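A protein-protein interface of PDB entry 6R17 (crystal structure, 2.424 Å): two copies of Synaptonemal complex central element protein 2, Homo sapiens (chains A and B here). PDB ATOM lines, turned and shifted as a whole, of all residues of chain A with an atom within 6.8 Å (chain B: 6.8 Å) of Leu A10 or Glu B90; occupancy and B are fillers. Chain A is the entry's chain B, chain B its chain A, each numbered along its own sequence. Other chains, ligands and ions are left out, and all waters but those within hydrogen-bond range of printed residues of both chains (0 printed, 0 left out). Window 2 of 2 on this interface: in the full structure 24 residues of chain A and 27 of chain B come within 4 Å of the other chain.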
ATOM      1  N   LEU A   5       7.716   7.371   2.080  1.00  0.00           N
ATOM      2  CA  LEU A   5       6.317   7.784   2.137  1.00  0.00           C
ATOM      3  C   LEU A   5       5.694   7.799   0.745  1.00  0.00           C
ATOM      4  O   LEU A   5       4.548   7.367   0.567  1.00  0.00           O
ATOM      5  CB  LEU A   5       6.190   9.150   2.813  1.00  0.00           C
ATOM      6  CG  LEU A   5       4.762   9.655   3.047  1.00  0.00           C
ATOM      7  CD1 LEU A   5       3.969   8.646   3.861  1.00  0.00           C
ATOM      8  CD2 LEU A   5       4.769  11.006   3.748  1.00  0.00           C
ATOM      9  N   TYR A   6       6.428   8.299  -0.253  1.00  0.00           N
ATOM     10  CA  TYR A   6       5.916   8.290  -1.620  1.00  0.00           C
ATOM     11  C   TYR A   6       5.686   6.868  -2.121  1.00  0.00           C
ATOM     12  O   TYR A   6       4.663   6.589  -2.758  1.00  0.00           O
ATOM     13  CB  TYR A   6       6.882   9.027  -2.551  1.00  0.00           C
ATOM     14  CG  TYR A   6       7.066  10.499  -2.249  1.00  0.00           C
ATOM     15  CD1 TYR A   6       6.227  11.453  -2.811  1.00  0.00           C
ATOM     16  CD2 TYR A   6       8.083  10.936  -1.411  1.00  0.00           C
ATOM     17  CE1 TYR A   6       6.392  12.799  -2.544  1.00  0.00           C
ATOM     18  CE2 TYR A   6       8.256  12.282  -1.136  1.00  0.00           C
ATOM     19  CZ  TYR A   6       7.407  13.208  -1.705  1.00  0.00           C
ATOM     20  OH  TYR A   6       7.575  14.548  -1.437  1.00  0.00           O
ATOM     21  N   PHE A   7       6.625   5.954  -1.851  1.00  0.00           N
ATOM     22  CA  PHE A   7       6.432   4.570  -2.277  1.00  0.00           C
ATOM     23  C   PHE A   7       5.225   3.932  -1.599  1.00  0.00           C
ATOM     24  O   PHE A   7       4.459   3.209  -2.244  1.00  0.00           O
ATOM     25  CB  PHE A   7       7.689   3.731  -2.029  1.00  0.00           C
ATOM     26  CG  PHE A   7       8.766   3.925  -3.062  1.00  0.00           C
ATOM     27  CD1 PHE A   7       8.575   3.469  -4.358  1.00  0.00           C
ATOM     28  CD2 PHE A   7       9.974   4.521  -2.738  1.00  0.00           C
ATOM     29  CE1 PHE A   7       9.553   3.627  -5.319  1.00  0.00           C
ATOM     30  CE2 PHE A   7      10.961   4.679  -3.699  1.00  0.00           C
ATOM     31  CZ  PHE A   7      10.749   4.230  -4.990  1.00  0.00           C
ATOM     32  N   SER A   8       5.035   4.181  -0.300  1.00  0.00           N
ATOM     33  CA  SER A   8       3.884   3.601   0.389  1.00  0.00           C
ATOM     34  C   SER A   8       2.572   4.199  -0.112  1.00  0.00           C
ATOM     35  O   SER A   8       1.572   3.485  -0.253  1.00  0.00           O
ATOM     36  CB  SER A   8       4.024   3.794   1.898  1.00  0.00           C
ATOM     37  OG  SER A   8       4.033   5.169   2.239  1.00  0.00           O
ATOM     38  N   SER A   9       2.565   5.499  -0.409  1.00  0.00           N
ATOM     39  CA  SER A   9       1.375   6.127  -0.978  1.00  0.00           C
ATOM     40  C   SER A   9       1.041   5.527  -2.339  1.00  0.00           C
ATOM     41  O   SER A   9      -0.121   5.215  -2.633  1.00  0.00           O
ATOM     42  CB  SER A   9       1.587   7.638  -1.083  1.00  0.00           C
ATOM     43  OG  SER A   9       0.594   8.243  -1.891  1.00  0.00           O
ATOM     44  N   LEU A  10       2.056   5.360  -3.187  1.00  0.00           N
ATOM     45  CA  LEU A  10       1.829   4.780  -4.504  1.00  0.00           C
ATOM     46  C   LEU A  10       1.426   3.313  -4.421  1.00  0.00           C
ATOM     47  O   LEU A  10       0.609   2.849  -5.224  1.00  0.00           O
ATOM     48  CB  LEU A  10       3.091   4.944  -5.343  1.00  0.00           C
ATOM     49  CG  LEU A  10       3.182   4.146  -6.634  1.00  0.00           C
ATOM     50  CD1 LEU A  10       2.093   4.586  -7.577  1.00  0.00           C
ATOM     51  CD2 LEU A  10       4.542   4.360  -7.240  1.00  0.00           C
ATOM     52  N   ASP A  11       1.937   2.582  -3.428  1.00  0.00           N
ATOM     53  CA  ASP A  11       1.499   1.206  -3.223  1.00  0.00           C
ATOM     54  C   ASP A  11       0.046   1.154  -2.781  1.00  0.00           C
ATOM     55  O   ASP A  11      -0.709   0.276  -3.213  1.00  0.00           O
ATOM     56  CB  ASP A  11       2.397   0.509  -2.200  1.00  0.00           C
ATOM     57  CG  ASP A  11       3.760   0.166  -2.760  1.00  0.00           C
ATOM     58  OD1 ASP A  11       3.866  -0.010  -3.989  1.00  0.00           O
ATOM     59  OD2 ASP A  11       4.726   0.080  -1.972  1.00  0.00           O
ATOM     60  N   SER A  12      -0.365   2.090  -1.924  1.00  0.00           N
ATOM     61  CA  SER A  12      -1.763   2.137  -1.518  1.00  0.00           C
ATOM     62  C   SER A  12      -2.671   2.469  -2.697  1.00  0.00           C
ATOM     63  O   SER A  12      -3.744   1.878  -2.842  1.00  0.00           O
ATOM     64  CB  SER A  12      -1.947   3.156  -0.393  1.00  0.00           C
ATOM     65  OG  SER A  12      -3.292   3.192   0.046  1.00  0.00           O
ATOM     66  N   SER A  13      -2.239   3.382  -3.571  1.00  0.00           N
ATOM     67  CA  SER A  13      -3.015   3.668  -4.778  1.00  0.00           C
ATOM     68  C   SER A  13      -3.120   2.441  -5.680  1.00  0.00           C
ATOM     69  O   SER A  13      -4.206   2.112  -6.184  1.00  0.00           O
ATOM     70  CB  SER A  13      -2.389   4.836  -5.538  1.00  0.00           C
ATOM     71  OG  SER A  13      -2.558   6.053  -4.831  1.00  0.00           O
ATOM     72  N   ILE A  14      -2.005   1.733  -5.870  1.00  0.00           N
ATOM     73  CA  ILE A  14      -2.009   0.537  -6.708  1.00  0.00           C
ATOM     74  C   ILE A  14      -2.945  -0.517  -6.133  1.00  0.00           C
ATOM     75  O   ILE A  14      -3.706  -1.164  -6.868  1.00  0.00           O
ATOM     76  CB  ILE A  14      -0.572   0.005  -6.873  1.00  0.00           C
ATOM     77  CG1 ILE A  14       0.260   0.962  -7.736  1.00  0.00           C
ATOM     78  CG2 ILE A  14      -0.563  -1.416  -7.412  1.00  0.00           C
ATOM     79  CD1 ILE A  14       1.735   0.622  -7.784  1.00  0.00           C
ATOM     80  N   ASP A  15      -2.907  -0.717  -4.815  1.00  0.00           N
ATOM     81  CA  ASP A  15      -3.813  -1.686  -4.212  1.00  0.00           C
ATOM     82  C   ASP A  15      -5.269  -1.257  -4.334  1.00  0.00           C
ATOM     83  O   ASP A  15      -6.150  -2.108  -4.489  1.00  0.00           O
ATOM     84  CB  ASP A  15      -3.481  -1.950  -2.757  1.00  0.00           C
ATOM     85  CG  ASP A  15      -4.384  -3.013  -2.174  1.00  0.00           C
ATOM     86  OD1 ASP A  15      -4.173  -4.207  -2.472  1.00  0.00           O
ATOM     87  OD2 ASP A  15      -5.305  -2.652  -1.410  1.00  0.00           O
ATOM     88  N   LYS B  85       2.975  -3.566 -15.664  1.00  0.00           N
ATOM     89  CA  LYS B  85       3.998  -2.633 -16.124  1.00  0.00           C
ATOM     90  C   LYS B  85       4.316  -1.614 -15.038  1.00  0.00           C
ATOM     91  O   LYS B  85       5.487  -1.298 -14.790  1.00  0.00           O
ATOM     92  CB  LYS B  85       3.528  -1.949 -17.409  1.00  0.00           C
ATOM     93  CG  LYS B  85       4.482  -0.920 -17.991  1.00  0.00           C
ATOM     94  CD  LYS B  85       3.982  -0.452 -19.352  1.00  0.00           C
ATOM     95  CE  LYS B  85       4.627   0.850 -19.787  1.00  0.00           C
ATOM     96  NZ  LYS B  85       4.203   1.227 -21.165  1.00  0.00           N
ATOM     97  N   ILE B  86       3.283  -1.122 -14.351  1.00  0.00           N
ATOM     98  CA  ILE B  86       3.499  -0.161 -13.273  1.00  0.00           C
ATOM     99  C   ILE B  86       4.229  -0.813 -12.108  1.00  0.00           C
ATOM    100  O   ILE B  86       5.110  -0.204 -11.490  1.00  0.00           O
ATOM    101  CB  ILE B  86       2.156   0.430 -12.816  1.00  0.00           C
ATOM    102  CG1 ILE B  86       1.589   1.376 -13.864  1.00  0.00           C
ATOM    103  CG2 ILE B  86       2.299   1.131 -11.473  1.00  0.00           C
ATOM    104  CD1 ILE B  86       0.275   1.934 -13.447  1.00  0.00           C
ATOM    105  N   SER B  87       3.877  -2.060 -11.791  1.00  0.00           N
ATOM    106  CA  SER B  87       4.548  -2.768 -10.705  1.00  0.00           C
ATOM    107  C   SER B  87       6.032  -2.934 -11.001  1.00  0.00           C
ATOM    108  O   SER B  87       6.884  -2.693 -10.137  1.00  0.00           O
ATOM    109  CB  SER B  87       3.880  -4.126 -10.480  1.00  0.00           C
ATOM    110  OG  SER B  87       4.775  -5.046  -9.884  1.00  0.00           O
ATOM    111  N   HIS B  88       6.361  -3.330 -12.232  1.00  0.00           N
ATOM    112  CA  HIS B  88       7.761  -3.496 -12.610  1.00  0.00           C
ATOM    113  C   HIS B  88       8.506  -2.165 -12.579  1.00  0.00           C
ATOM    114  O   HIS B  88       9.639  -2.084 -12.078  1.00  0.00           O
ATOM    115  CB  HIS B  88       7.843  -4.135 -13.996  1.00  0.00           C
ATOM    116  CG  HIS B  88       9.220  -4.148 -14.579  1.00  0.00           C
ATOM    117  ND1 HIS B  88      10.251  -4.886 -14.038  1.00  0.00           N
ATOM    118  CD2 HIS B  88       9.735  -3.521 -15.664  1.00  0.00           C
ATOM    119  CE1 HIS B  88      11.343  -4.709 -14.762  1.00  0.00           C
ATOM    120  NE2 HIS B  88      11.056  -3.886 -15.754  1.00  0.00           N
ATOM    121  N   LEU B  89       7.874  -1.105 -13.090  1.00  0.00           N
ATOM    122  CA  LEU B  89       8.489   0.219 -13.063  1.00  0.00           C
ATOM    123  C   LEU B  89       8.778   0.661 -11.633  1.00  0.00           C
ATOM    124  O   LEU B  89       9.864   1.173 -11.327  1.00  0.00           O
ATOM    125  CB  LEU B  89       7.560   1.223 -13.748  1.00  0.00           C
ATOM    126  CG  LEU B  89       7.572   1.327 -15.272  1.00  0.00           C
ATOM    127  CD1 LEU B  89       6.384   2.154 -15.742  1.00  0.00           C
ATOM    128  CD2 LEU B  89       8.876   1.922 -15.768  1.00  0.00           C
ATOM    129  N   GLU B  90       7.802   0.478 -10.743  1.00  0.00           N
ATOM    130  CA  GLU B  90       7.970   0.902  -9.360  1.00  0.00           C
ATOM    131  C   GLU B  90       9.030   0.070  -8.647  1.00  0.00           C
ATOM    132  O   GLU B  90       9.754   0.588  -7.792  1.00  0.00           O
ATOM    133  CB  GLU B  90       6.628   0.859  -8.633  1.00  0.00           C
ATOM    134  CG  GLU B  90       6.677   1.551  -7.292  1.00  0.00           C
ATOM    135  CD  GLU B  90       5.771   0.926  -6.267  1.00  0.00           C
ATOM    136  OE1 GLU B  90       5.469  -0.282  -6.379  1.00  0.00           O
ATOM    137  OE2 GLU B  90       5.359   1.660  -5.345  1.00  0.00           O
ATOM    138  N   THR B  91       9.121  -1.229  -8.955  1.00  0.00           N
ATOM    139  CA  THR B  91      10.206  -2.029  -8.388  1.00  0.00           C
ATOM    140  C   THR B  91      11.564  -1.509  -8.853  1.00  0.00           C
ATOM    141  O   THR B  91      12.525  -1.464  -8.071  1.00  0.00           O
ATOM    142  CB  THR B  91      10.045  -3.502  -8.763  1.00  0.00           C
ATOM    143  OG1 THR B  91       9.897  -3.624 -10.183  1.00  0.00           O
ATOM    144  CG2 THR B  91       8.830  -4.102  -8.070  1.00  0.00           C
ATOM    145  N   GLU B  92      11.662  -1.121 -10.128  1.00  0.00           N
ATOM    146  CA  GLU B  92      12.891  -0.504 -10.621  1.00  0.00           C
ATOM    147  C   GLU B  92      13.225   0.755  -9.826  1.00  0.00           C
ATOM    148  O   GLU B  92      14.374   0.963  -9.411  1.00  0.00           O
ATOM    149  CB  GLU B  92      12.760  -0.180 -12.108  1.00  0.00           C
ATOM    150  CG  GLU B  92      13.324  -1.244 -13.033  1.00  0.00           C
ATOM    151  CD  GLU B  92      13.034  -0.955 -14.493  1.00  0.00           C
ATOM    152  OE1 GLU B  92      13.086   0.229 -14.887  1.00  0.00           O
ATOM    153  OE2 GLU B  92      12.755  -1.911 -15.247  1.00  0.00           O
ATOM    154  N   LEU B  93      12.222   1.609  -9.603  1.00  0.00           N
ATOM    155  CA  LEU B  93      12.457   2.840  -8.854  1.00  0.00           C
ATOM    156  C   LEU B  93      12.871   2.533  -7.420  1.00  0.00           C
ATOM    157  O   LEU B  93      13.711   3.235  -6.843  1.00  0.00           O
ATOM    158  CB  LEU B  93      11.209   3.721  -8.868  1.00  0.00           C
ATOM    159  CG  LEU B  93      10.723   4.181 -10.239  1.00  0.00           C
ATOM    160  CD1 LEU B  93       9.650   5.239 -10.080  1.00  0.00           C
ATOM    161  CD2 LEU B  93      11.881   4.713 -11.064  1.00  0.00           C
ATOM    162  N   LYS B  94      12.274   1.500  -6.827  1.00  0.00           N
ATOM    163  CA  LYS B  94      12.687   1.044  -5.505  1.00  0.00           C
ATOM    164  C   LYS B  94      14.165   0.682  -5.502  1.00  0.00           C
ATOM    165  O   LYS B  94      14.905   1.049  -4.581  1.00  0.00           O
ATOM    166  CB  LYS B  94      11.822  -0.136  -5.060  1.00  0.00           C
ATOM    167  CG  LYS B  94      10.491   0.300  -4.464  1.00  0.00           C
ATOM    168  CD  LYS B  94       9.715  -0.860  -3.865  1.00  0.00           C
ATOM    169  CE  LYS B  94       8.259  -0.476  -3.634  1.00  0.00           C
ATOM    170  NZ  LYS B  94       7.343  -1.649  -3.691  1.00  0.00           N
ATOM    171  N   GLN B  95      14.609  -0.067  -6.518  1.00  0.00           N
ATOM    172  CA  GLN B  95      16.026  -0.413  -6.604  1.00  0.00           C
ATOM    173  C   GLN B  95      16.888   0.839  -6.674  1.00  0.00           C
ATOM    174  O   GLN B  95      17.897   0.956  -5.967  1.00  0.00           O
ATOM    175  CB  GLN B  95      16.313  -1.238  -7.856  1.00  0.00           C
ATOM    176  CG  GLN B  95      15.882  -2.669  -7.899  1.00  0.00           C
ATOM    177  CD  GLN B  95      16.447  -3.337  -9.137  1.00  0.00           C
ATOM    178  OE1 GLN B  95      17.658  -3.538  -9.246  1.00  0.00           O
ATOM    179  NE2 GLN B  95      15.581  -3.652 -10.093  1.00  0.00           N
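The side-chain carboxylate (OD1) of Asp A11 lies close to the side-chain carboxylate (OE2) of Glu B90 (2.6 Å).
OD2 of Asp A11 lies within salt-bridge range of NZ of Lys B94 (3.6 Å).
The side-chain carboxylate (OE1) of Glu B90 is in salt-bridge range of the side-chain amino group (NZ) of Lys B94 (3.6 Å).
Among the printed residues, merely in contact across the chains: Phe A7 with Glu B90 (3.6 Å), Phe A7 with Leu B93 (3.6 Å), Phe A7 with Lys B94 (3.6 Å), Leu A10 with Glu B90 (3.4 Å) and Ile A14 with Ile B86 (3.8 Å).
Glu B90 touches just these residues of chain A: Phe A7, Leu A10 and Asp A11.
Printed residues of chain A within 4 Å of Ile B86: Ile A14.
Printed residues of chain B within 4 Å of Ile A14: Ile B86.
Of the 11 printed residues of chain A, 4 touch a printed residue of chain B.
Hydrophobic or aromatic side chains of chain A that line the printed part of chain B: Phe A7, Leu A10 and Ile A14.
Among the printed residues, Asp or Glu carboxylates within 4 Å of a Lys or Arg side-chain nitrogen of the other chain: Asp A11 with Lys B94.
No position is printed for both chains.
Of the 7 pairs that touch across the chains among the printed residues, none has its exchanged pair printed and touching as well.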
